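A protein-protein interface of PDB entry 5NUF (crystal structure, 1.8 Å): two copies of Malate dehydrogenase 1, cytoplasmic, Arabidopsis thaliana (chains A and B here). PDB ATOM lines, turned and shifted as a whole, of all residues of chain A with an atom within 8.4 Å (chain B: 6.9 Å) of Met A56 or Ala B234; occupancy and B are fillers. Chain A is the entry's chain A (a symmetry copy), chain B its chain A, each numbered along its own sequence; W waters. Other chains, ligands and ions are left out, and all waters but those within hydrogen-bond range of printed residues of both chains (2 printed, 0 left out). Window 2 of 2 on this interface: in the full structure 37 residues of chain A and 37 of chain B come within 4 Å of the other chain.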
ATOM      1  N   MET A  41      -9.219   1.727  -1.808  1.00  0.00           N
ATOM      2  CA  MET A  41     -10.067   2.173  -0.719  1.00  0.00           C
ATOM      3  C   MET A  41     -11.471   1.828  -1.115  1.00  0.00           C
ATOM      4  O   MET A  41     -11.919   2.267  -2.193  1.00  0.00           O
ATOM      5  CB  MET A  41      -9.901   3.680  -0.556  1.00  0.00           C
ATOM      6  CG  MET A  41      -8.507   4.053  -0.080  1.00  0.00           C
ATOM      7  SD  MET A  41      -8.511   5.738   0.604  1.00  0.00           S
ATOM      8  CE  MET A  41      -9.097   6.777  -0.723  1.00  0.00           C
ATOM      9  N   GLU A  49     -18.848  10.580  -1.895  1.00  0.00           N
ATOM     10  CA  GLU A  49     -18.233  11.906  -1.914  1.00  0.00           C
ATOM     11  C   GLU A  49     -17.087  11.970  -0.895  1.00  0.00           C
ATOM     12  O   GLU A  49     -15.970  12.473  -1.192  1.00  0.00           O
ATOM     13  CB  GLU A  49     -19.285  13.022  -1.670  1.00  0.00           C
ATOM     14  CG  GLU A  49     -20.267  13.198  -2.831  1.00  0.00           C
ATOM     15  CD  GLU A  49     -19.585  13.896  -4.024  1.00  0.00           C
ATOM     16  OE1 GLU A  49     -18.492  14.566  -3.874  1.00  0.00           O
ATOM     17  OE2 GLU A  49     -20.124  13.760  -5.114  1.00  0.00           O
ATOM     18  N   ALA A  50     -17.356  11.504   0.306  1.00  0.00           N
ATOM     19  CA  ALA A  50     -16.333  11.522   1.396  1.00  0.00           C
ATOM     20  C   ALA A  50     -15.110  10.679   0.966  1.00  0.00           C
ATOM     21  O   ALA A  50     -13.971  11.093   1.178  1.00  0.00           O
ATOM     22  CB  ALA A  50     -16.873  11.014   2.702  1.00  0.00           C
ATOM     23  N   LEU A  51     -15.357   9.570   0.297  1.00  0.00           N
ATOM     24  CA  LEU A  51     -14.296   8.731  -0.121  1.00  0.00           C
ATOM     25  C   LEU A  51     -13.380   9.399  -1.156  1.00  0.00           C
ATOM     26  O   LEU A  51     -12.141   9.318  -1.086  1.00  0.00           O
ATOM     27  CB  LEU A  51     -14.856   7.458  -0.688  1.00  0.00           C
ATOM     28  CG  LEU A  51     -13.996   6.323  -1.105  1.00  0.00           C
ATOM     29  CD1 LEU A  51     -13.139   5.862   0.018  1.00  0.00           C
ATOM     30  CD2 LEU A  51     -14.992   5.213  -1.558  1.00  0.00           C
ATOM     31  N   ASN A  52     -13.981  10.054  -2.109  1.00  0.00           N
ATOM     32  CA  ASN A  52     -13.256  10.816  -3.116  1.00  0.00           C
ATOM     33  C   ASN A  52     -12.453  11.917  -2.385  1.00  0.00           C
ATOM     34  O   ASN A  52     -11.302  12.230  -2.736  1.00  0.00           O
ATOM     35  CB  ASN A  52     -14.222  11.451  -4.137  1.00  0.00           C
ATOM     36  CG  ASN A  52     -13.480  12.340  -5.125  1.00  0.00           C
ATOM     37  OD1 ASN A  52     -12.531  11.907  -5.821  1.00  0.00           O
ATOM     38  ND2 ASN A  52     -13.799  13.628  -5.074  1.00  0.00           N
ATOM     39  N   GLY A  53     -13.058  12.495  -1.327  1.00  0.00           N
ATOM     40  CA  GLY A  53     -12.367  13.476  -0.500  1.00  0.00           C
ATOM     41  C   GLY A  53     -11.049  12.972   0.121  1.00  0.00           C
ATOM     42  O   GLY A  53     -10.007  13.645   0.130  1.00  0.00           O
ATOM     43  N   VAL A  54     -11.146  11.748   0.610  1.00  0.00           N
ATOM     44  CA  VAL A  54      -9.949  11.084   1.132  1.00  0.00           C
ATOM     45  C   VAL A  54      -8.879  10.896   0.076  1.00  0.00           C
ATOM     46  O   VAL A  54      -7.716  11.159   0.332  1.00  0.00           O
ATOM     47  CB  VAL A  54     -10.288   9.782   1.851  1.00  0.00           C
ATOM     48  CG1 VAL A  54      -9.025   9.154   2.409  1.00  0.00           C
ATOM     49  CG2 VAL A  54     -11.295  10.044   2.939  1.00  0.00           C
ATOM     50  N   LYS A  55      -9.276  10.447  -1.100  1.00  0.00           N
ATOM     51  CA  LYS A  55      -8.323  10.277  -2.200  1.00  0.00           C
ATOM     52  C   LYS A  55      -7.675  11.638  -2.533  1.00  0.00           C
ATOM     53  O   LYS A  55      -6.459  11.704  -2.751  1.00  0.00           O
ATOM     54  CB  LYS A  55      -9.028   9.733  -3.453  1.00  0.00           C
ATOM     55  CG  LYS A  55      -8.124   9.684  -4.670  1.00  0.00           C
ATOM     56  CD  LYS A  55      -8.659   8.950  -5.843  1.00  0.00           C
ATOM     57  CE  LYS A  55      -7.587   9.092  -6.938  1.00  0.00           C
ATOM     58  NZ  LYS A  55      -7.713   8.244  -8.105  1.00  0.00           N
ATOM     59  N   MET A  56      -8.494  12.679  -2.616  1.00  0.00           N
ATOM     60  CA  MET A  56      -7.970  14.055  -2.898  1.00  0.00           C
ATOM     61  C   MET A  56      -6.892  14.418  -1.873  1.00  0.00           C
ATOM     62  O   MET A  56      -5.834  14.910  -2.240  1.00  0.00           O
ATOM     63  CB  MET A  56      -9.117  15.096  -2.879  1.00  0.00           C
ATOM     64  CG  MET A  56     -10.075  15.055  -4.076  1.00  0.00           C
ATOM     65  SD  MET A  56     -11.583  16.002  -3.706  1.00  0.00           S
ATOM     66  CE  MET A  56     -10.868  17.543  -4.184  1.00  0.00           C
ATOM     67  N   GLU A  57      -7.146  14.104  -0.616  1.00  0.00           N
ATOM     68  CA  GLU A  57      -6.144  14.411   0.436  1.00  0.00           C
ATOM     69  C   GLU A  57      -4.878  13.596   0.277  1.00  0.00           C
ATOM     70  O   GLU A  57      -3.781  14.105   0.541  1.00  0.00           O
ATOM     71  CB  GLU A  57      -6.731  14.215   1.843  1.00  0.00           C
ATOM     72  CG  GLU A  57      -7.693  15.367   2.199  1.00  0.00           C
ATOM     73  CD  GLU A  57      -7.774  15.570   3.684  1.00  0.00           C
ATOM     74  OE1 GLU A  57      -6.754  16.029   4.282  1.00  0.00           O
ATOM     75  OE2 GLU A  57      -8.850  15.257   4.278  1.00  0.00           O
ATOM     76  N   LEU A  58      -5.023  12.296  -0.123  1.00  0.00           N
ATOM     77  CA  LEU A  58      -3.868  11.463  -0.286  1.00  0.00           C
ATOM     78  C   LEU A  58      -2.995  11.991  -1.417  1.00  0.00           C
ATOM     79  O   LEU A  58      -1.766  11.992  -1.315  1.00  0.00           O
ATOM     80  CB  LEU A  58      -4.303  10.037  -0.592  1.00  0.00           C
ATOM     81  CG  LEU A  58      -4.888   9.230   0.584  1.00  0.00           C
ATOM     82  CD1 LEU A  58      -5.554   7.964   0.130  1.00  0.00           C
ATOM     83  CD2 LEU A  58      -3.765   8.835   1.543  1.00  0.00           C
ATOM     84  N   ILE A  59      -3.629  12.452  -2.492  1.00  0.00           N
ATOM     85  CA  ILE A  59      -2.903  13.089  -3.599  1.00  0.00           C
ATOM     86  C   ILE A  59      -2.232  14.355  -3.118  1.00  0.00           C
ATOM     87  O   ILE A  59      -1.086  14.596  -3.456  1.00  0.00           O
ATOM     88  CB  ILE A  59      -3.891  13.394  -4.751  1.00  0.00           C
ATOM     89  CG1 ILE A  59      -4.224  12.074  -5.464  1.00  0.00           C
ATOM     90  CG2 ILE A  59      -3.351  14.396  -5.736  1.00  0.00           C
ATOM     91  CD1 ILE A  59      -5.498  12.236  -6.276  1.00  0.00           C
ATOM     92  N   ASP A  60      -2.969  15.152  -2.338  1.00  0.00           N
ATOM     93  CA  ASP A  60      -2.502  16.428  -1.850  1.00  0.00           C
ATOM     94  C   ASP A  60      -1.308  16.339  -0.906  1.00  0.00           C
ATOM     95  O   ASP A  60      -0.584  17.320  -0.766  1.00  0.00           O
ATOM     96  CB  ASP A  60      -3.633  17.199  -1.163  1.00  0.00           C
ATOM     97  CG  ASP A  60      -4.701  17.656  -2.106  1.00  0.00           C
ATOM     98  OD1 ASP A  60      -4.561  17.521  -3.341  1.00  0.00           O
ATOM     99  OD2 ASP A  60      -5.730  18.154  -1.593  1.00  0.00           O
ATOM    100  N   ALA A  61      -1.106  15.189  -0.275  1.00  0.00           N
ATOM    101  CA  ALA A  61       0.024  14.976   0.627  1.00  0.00           C
ATOM    102  C   ALA A  61       1.347  14.676  -0.063  1.00  0.00           C
ATOM    103  O   ALA A  61       2.426  14.698   0.589  1.00  0.00           O
ATOM    104  CB  ALA A  61      -0.321  13.844   1.599  1.00  0.00           C
ATOM    105  N   ALA A  62       1.286  14.373  -1.371  1.00  0.00           N
ATOM    106  CA  ALA A  62       2.517  14.112  -2.143  1.00  0.00           C
ATOM    107  C   ALA A  62       3.430  13.062  -1.444  1.00  0.00           C
ATOM    108  O   ALA A  62       4.606  13.284  -1.168  1.00  0.00           O
ATOM    109  CB  ALA A  62       3.305  15.410  -2.389  1.00  0.00           C
ATOM    110  N   PHE A  63       2.822  11.914  -1.125  1.00  0.00           N
ATOM    111  CA  PHE A  63       3.492  10.816  -0.500  1.00  0.00           C
ATOM    112  C   PHE A  63       4.431  10.091  -1.527  1.00  0.00           C
ATOM    113  O   PHE A  63       3.936   9.469  -2.480  1.00  0.00           O
ATOM    114  CB  PHE A  63       2.462   9.764  -0.027  1.00  0.00           C
ATOM    115  CG  PHE A  63       1.650  10.153   1.193  1.00  0.00           C
ATOM    116  CD1 PHE A  63       2.252  10.309   2.437  1.00  0.00           C
ATOM    117  CD2 PHE A  63       0.273  10.316   1.094  1.00  0.00           C
ATOM    118  CE1 PHE A  63       1.497  10.669   3.529  1.00  0.00           C
ATOM    119  CE2 PHE A  63      -0.472  10.615   2.189  1.00  0.00           C
ATOM    120  CZ  PHE A  63       0.121  10.779   3.393  1.00  0.00           C
ATOM    121  N   VAL A  69      -4.038   5.398  -6.224  1.00  0.00           N
ATOM    122  CA  VAL A  69      -5.115   5.281  -5.297  1.00  0.00           C
ATOM    123  C   VAL A  69      -6.408   4.996  -6.072  1.00  0.00           C
ATOM    124  O   VAL A  69      -6.815   5.782  -6.919  1.00  0.00           O
ATOM    125  CB  VAL A  69      -5.325   6.595  -4.525  1.00  0.00           C
ATOM    126  CG1 VAL A  69      -6.480   6.456  -3.573  1.00  0.00           C
ATOM    127  CG2 VAL A  69      -4.043   7.013  -3.791  1.00  0.00           C
ATOM    128  N   ALA A  71     -10.301   4.590  -5.384  1.00  0.00           N
ATOM    129  CA  ALA A  71     -11.281   4.908  -4.357  1.00  0.00           C
ATOM    130  C   ALA A  71     -12.649   4.588  -4.921  1.00  0.00           C
ATOM    131  O   ALA A  71     -13.086   5.238  -5.876  1.00  0.00           O
ATOM    132  CB  ALA A  71     -11.160   6.397  -3.991  1.00  0.00           C
ATOM    133  N   ARG B 163       0.084  20.024  -2.716  1.00  0.00           N
ATOM    134  CA  ARG B 163      -1.062  20.022  -3.594  1.00  0.00           C
ATOM    135  C   ARG B 163      -0.643  20.273  -5.014  1.00  0.00           C
ATOM    136  O   ARG B 163      -1.172  19.647  -5.956  1.00  0.00           O
ATOM    137  CB  ARG B 163      -2.110  21.059  -3.171  1.00  0.00           C
ATOM    138  CG  ARG B 163      -3.013  20.567  -2.067  1.00  0.00           C
ATOM    139  CD  ARG B 163      -3.693  21.745  -1.385  1.00  0.00           C
ATOM    140  NE  ARG B 163      -4.651  21.309  -0.396  1.00  0.00           N
ATOM    141  CZ  ARG B 163      -5.270  22.141   0.468  1.00  0.00           C
ATOM    142  NH1 ARG B 163      -4.988  23.432   0.521  1.00  0.00           N
ATOM    143  NH2 ARG B 163      -6.117  21.665   1.387  1.00  0.00           N
ATOM    144  N   THR B 227      -7.089  25.773  -9.409  1.00  0.00           N
ATOM    145  CA  THR B 227      -7.251  24.514  -8.717  1.00  0.00           C
ATOM    146  C   THR B 227      -6.463  24.484  -7.371  1.00  0.00           C
ATOM    147  O   THR B 227      -7.027  24.070  -6.328  1.00  0.00           O
ATOM    148  CB  THR B 227      -6.840  23.331  -9.608  1.00  0.00           C
ATOM    149  OG1 THR B 227      -7.746  23.341 -10.728  1.00  0.00           O
ATOM    150  CG2 THR B 227      -6.955  21.988  -8.859  1.00  0.00           C
ATOM    151  N   GLN B 230      -8.003  26.972  -4.824  1.00  0.00           N
ATOM    152  CA  GLN B 230      -9.329  26.617  -4.346  1.00  0.00           C
ATOM    153  C   GLN B 230      -9.375  25.220  -3.740  1.00  0.00           C
ATOM    154  O   GLN B 230     -10.407  24.752  -3.382  1.00  0.00           O
ATOM    155  CB  GLN B 230     -10.351  26.745  -5.500  1.00  0.00           C
ATOM    156  CG  GLN B 230     -10.510  28.194  -6.032  1.00  0.00           C
ATOM    157  CD  GLN B 230     -11.004  29.127  -4.972  1.00  0.00           C
ATOM    158  OE1 GLN B 230     -11.772  28.721  -4.046  1.00  0.00           O
ATOM    159  NE2 GLN B 230     -10.508  30.400  -5.009  1.00  0.00           N
ATOM    160  N   ARG B 231      -8.250  24.559  -3.633  1.00  0.00           N
ATOM    161  CA  ARG B 231      -8.208  23.142  -3.246  1.00  0.00           C
ATOM    162  C   ARG B 231      -8.733  22.889  -1.841  1.00  0.00           C
ATOM    163  O   ARG B 231      -9.518  21.959  -1.645  1.00  0.00           O
ATOM    164  CB  ARG B 231      -6.819  22.556  -3.450  1.00  0.00           C
ATOM    165  CG  ARG B 231      -6.750  21.069  -3.183  1.00  0.00           C
ATOM    166  CD  ARG B 231      -7.590  20.242  -4.131  1.00  0.00           C
ATOM    167  NE  ARG B 231      -7.092  18.878  -4.113  1.00  0.00           N
ATOM    168  CZ  ARG B 231      -7.357  17.919  -5.017  1.00  0.00           C
ATOM    169  NH1 ARG B 231      -8.155  18.143  -6.024  1.00  0.00           N
ATOM    170  NH2 ARG B 231      -6.741  16.773  -4.957  1.00  0.00           N
ATOM    171  N   GLY B 232      -8.414  23.762  -0.885  1.00  0.00           N
ATOM    172  CA  GLY B 232      -8.983  23.627   0.448  1.00  0.00           C
ATOM    173  C   GLY B 232     -10.534  23.688   0.467  1.00  0.00           C
ATOM    174  O   GLY B 232     -11.235  22.896   1.152  1.00  0.00           O
ATOM    175  N   ALA B 233     -11.088  24.610  -0.323  1.00  0.00           N
ATOM    176  CA  ALA B 233     -12.561  24.702  -0.454  1.00  0.00           C
ATOM    177  C   ALA B 233     -13.089  23.421  -1.108  1.00  0.00           C
ATOM    178  O   ALA B 233     -14.173  22.932  -0.789  1.00  0.00           O
ATOM    179  CB  ALA B 233     -12.957  25.906  -1.287  1.00  0.00           C
ATOM    180  N   ALA B 234     -12.333  22.862  -2.092  1.00  0.00           N
ATOM    181  CA  ALA B 234     -12.734  21.605  -2.715  1.00  0.00           C
ATOM    182  C   ALA B 234     -12.779  20.429  -1.738  1.00  0.00           C
ATOM    183  O   ALA B 234     -13.685  19.574  -1.794  1.00  0.00           O
ATOM    184  CB  ALA B 234     -11.940  21.267  -3.922  1.00  0.00           C
ATOM    185  N   ILE B 235     -11.868  20.391  -0.786  1.00  0.00           N
ATOM    186  CA  ILE B 235     -11.869  19.354   0.216  1.00  0.00           C
ATOM    187  C   ILE B 235     -13.125  19.483   1.072  1.00  0.00           C
ATOM    188  O   ILE B 235     -13.779  18.462   1.375  1.00  0.00           O
ATOM    189  CB  ILE B 235     -10.619  19.400   1.112  1.00  0.00           C
ATOM    190  CG1 ILE B 235      -9.329  19.128   0.307  1.00  0.00           C
ATOM    191  CG2 ILE B 235     -10.715  18.433   2.263  1.00  0.00           C
ATOM    192  CD1 ILE B 235      -9.262  17.860  -0.506  1.00  0.00           C
ATOM    193  N   ILE B 236     -13.452  20.718   1.478  1.00  0.00           N
ATOM    194  CA  ILE B 236     -14.635  20.965   2.291  1.00  0.00           C
ATOM    195  C   ILE B 236     -15.888  20.530   1.543  1.00  0.00           C
ATOM    196  O   ILE B 236     -16.791  19.981   2.151  1.00  0.00           O
ATOM    197  CB  ILE B 236     -14.743  22.456   2.702  1.00  0.00           C
ATOM    198  CG1 ILE B 236     -13.597  22.836   3.627  1.00  0.00           C
ATOM    199  CG2 ILE B 236     -16.099  22.785   3.318  1.00  0.00           C
ATOM    200  CD1 ILE B 236     -13.383  24.375   3.767  1.00  0.00           C
ATOM    201  N   LYS B 237     -15.952  20.804   0.243  1.00  0.00           N
ATOM    202  CA  LYS B 237     -17.113  20.403  -0.583  1.00  0.00           C
ATOM    203  C   LYS B 237     -17.238  18.849  -0.598  1.00  0.00           C
ATOM    204  O   LYS B 237     -18.333  18.329  -0.463  1.00  0.00           O
ATOM    205  CB  LYS B 237     -17.001  20.887  -2.025  1.00  0.00           C
ATOM    206  CG  LYS B 237     -17.267  22.370  -2.292  1.00  0.00           C
ATOM    207  CD  LYS B 237     -17.278  22.712  -3.788  1.00  0.00           C
ATOM    208  CE  LYS B 237     -17.897  24.117  -4.006  1.00  0.00           C
ATOM    209  NZ  LYS B 237     -17.886  24.546  -5.442  1.00  0.00           N
ATOM    210  N   ALA B 238     -16.122  18.136  -0.692  1.00  0.00           N
ATOM    211  CA  ALA B 238     -16.143  16.685  -0.773  1.00  0.00           C
ATOM    212  C   ALA B 238     -16.424  16.040   0.599  1.00  0.00           C
ATOM    213  O   ALA B 238     -17.166  15.082   0.678  1.00  0.00           O
ATOM    214  CB  ALA B 238     -14.821  16.188  -1.360  1.00  0.00           C
ATOM    215  N   ARG B 239     -15.830  16.568   1.666  1.00  0.00           N
ATOM    216  CA  ARG B 239     -15.844  15.928   2.963  1.00  0.00           C
ATOM    217  C   ARG B 239     -16.713  16.606   4.008  1.00  0.00           C
ATOM    218  O   ARG B 239     -16.943  16.047   5.051  1.00  0.00           O
ATOM    219  CB  ARG B 239     -14.402  15.865   3.561  1.00  0.00           C
ATOM    220  CG  ARG B 239     -13.430  15.029   2.759  1.00  0.00           C
ATOM    221  CD  ARG B 239     -12.066  14.941   3.380  1.00  0.00           C
ATOM    222  NE  ARG B 239     -12.213  14.465   4.754  1.00  0.00           N
ATOM    223  CZ  ARG B 239     -11.882  15.130   5.841  1.00  0.00           C
ATOM    224  NH1 ARG B 239     -11.173  16.270   5.779  1.00  0.00           N
ATOM    225  NH2 ARG B 239     -12.097  14.537   7.023  1.00  0.00           N
ATOM    226  N   LYS B 240     -17.152  17.815   3.763  1.00  0.00           N
ATOM    227  CA  LYS B 240     -17.882  18.642   4.760  1.00  0.00           C
ATOM    228  C   LYS B 240     -16.993  19.063   5.912  1.00  0.00           C
ATOM    229  O   LYS B 240     -17.512  19.531   6.904  1.00  0.00           O
ATOM    230  CB  LYS B 240     -19.173  17.942   5.257  1.00  0.00           C
ATOM    231  CG  LYS B 240     -20.099  17.417   4.139  1.00  0.00           C
ATOM    232  CD  LYS B 240     -20.216  18.436   2.995  1.00  0.00           C
ATOM    233  CE  LYS B 240     -21.441  18.334   2.069  1.00  0.00           C
ATOM    234  NZ  LYS B 240     -21.060  19.118   0.813  1.00  0.00           N
ATOM    235  N   LEU B 241     -15.662  18.946   5.748  1.00  0.00           N
ATOM    236  CA  LEU B 241     -14.675  19.285   6.765  1.00  0.00           C
ATOM    237  C   LEU B 241     -13.464  19.698   5.984  1.00  0.00           C
ATOM    238  O   LEU B 241     -13.251  19.216   4.885  1.00  0.00           O
ATOM    239  CB  LEU B 241     -14.302  18.092   7.623  1.00  0.00           C
ATOM    240  CG  LEU B 241     -15.398  17.483   8.512  1.00  0.00           C
ATOM    241  CD1 LEU B 241     -14.903  16.138   9.030  1.00  0.00           C
ATOM    242  CD2 LEU B 241     -15.742  18.479   9.615  1.00  0.00           C
ATOM    243  N   SER B 246      -3.937  15.394   5.157  1.00  0.00           N
ATOM    244  CA  SER B 246      -2.942  16.004   4.287  1.00  0.00           C
ATOM    245  C   SER B 246      -2.254  17.234   4.954  1.00  0.00           C
ATOM    246  O   SER B 246      -1.077  17.503   4.704  1.00  0.00           O
ATOM    247  CB  SER B 246      -3.577  16.378   2.941  1.00  0.00           C
ATOM    248  OG  SER B 246      -4.761  17.201   3.063  1.00  0.00           O
HETATM  249  O   HOH W   1      -3.531  18.418  -5.536  1.00  0.00           O
HETATM  250  O   HOH W   2      -5.848  18.753   0.971  1.00  0.00           O
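The side-chain hydroxyl of Ser B246 sits at hydrogen-bond distance from the side-chain carboxylate of Glu A57 (2.6 Å). NH2 of Arg B231 lies within hydrogen-bond range of O of Met A56, at 3.4 Å. The side-chain carboxylate (OE2) of Glu A57 lies within salt-bridge range of the guanidinium group (NH1) of Arg B239 (2.9 Å). OD1 of Asp A60 is in salt-bridge range of NH2 of Arg B231 (2.8 Å). OD2 of Asp A60 lies within salt-bridge range of NE of Arg B163 (3.5 Å). The backbone carbonyl oxygen of Ala B238 sits close to the backbone carbonyl oxygen of Glu A49.
The side-chain amide nitrogen (ND2) of Asn A52 lies within hydrogen-bond range of the side-chain sulfur (SD) of Met A56, 3.5 Å away.
Among the printed residues, pairs that only touch across the chains: Ala A50 with Ala B238, Met A56 with Ile B235, Asp A60 with Ile B235, Gly A53 with Ala B238, Gly A53 with Arg B239, Met A56 with Ala B234 and Glu A57 with Ile B235.
Ala B234 touches one residue of chain A. No residue of chain A comes within 4 Å of Gly B232. No residue of chain A comes within 4 Å of Ala B233. Of the printed residues of chain B, Glu A57 touches Ile B235 (3.999 Å), Arg B239 (2.9 Å) and Ser B246 (2.6 Å). Of the printed residues of chain B, Asp A60 touches Arg B163 (3.4 Å), Arg B231 (2.8 Å) and Ile B235 (3.7 Å). Of the printed residues of chain A, Ser B246 touches Glu A57 (2.6 Å). Ile A59 touches none of the printed residues of chain B. Ala A71 touches none of the printed residues of chain B. The nearest printed residue of chain B that does not touch Met A56 is Ala B238 (4.003 Å). The nearest residue of chain A that does not touch Ala B234 is Gly A53 (6.4 Å).
Of the 18 printed residues of chain A, 6 touch a printed residue of chain B. Hydrophobic or aromatic side chains of chain A that line the printed part of chain B: Met A56. Among the printed residues, 13 pairs touch across the chains. Among the printed residues, Asp or Glu carboxylates within 4 Å of a Lys or Arg side-chain nitrogen of the other chain: Glu A57 with Arg B239, Asp A60 with Arg B163 and Asp A60 with Arg B231.
No position is printed for both chains. Of the 13 pairs that touch across the chains among the printed residues, none has its exchanged pair printed and touching as well.
Water W1 bridges the side-chain carboxylate of Asp A60 (2.6 Å) and the backbone carbonyl oxygen of Arg B163 (2.7 Å). Water W2 lies within hydrogen-bond range of the side-chain carboxylate (OD2) of Asp A60 (2.6 Å), the side-chain hydroxyl (OG) of Ser B246 (2.8 Å) and the guanidinium group (NH2) of Arg B163 (3.0 Å).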
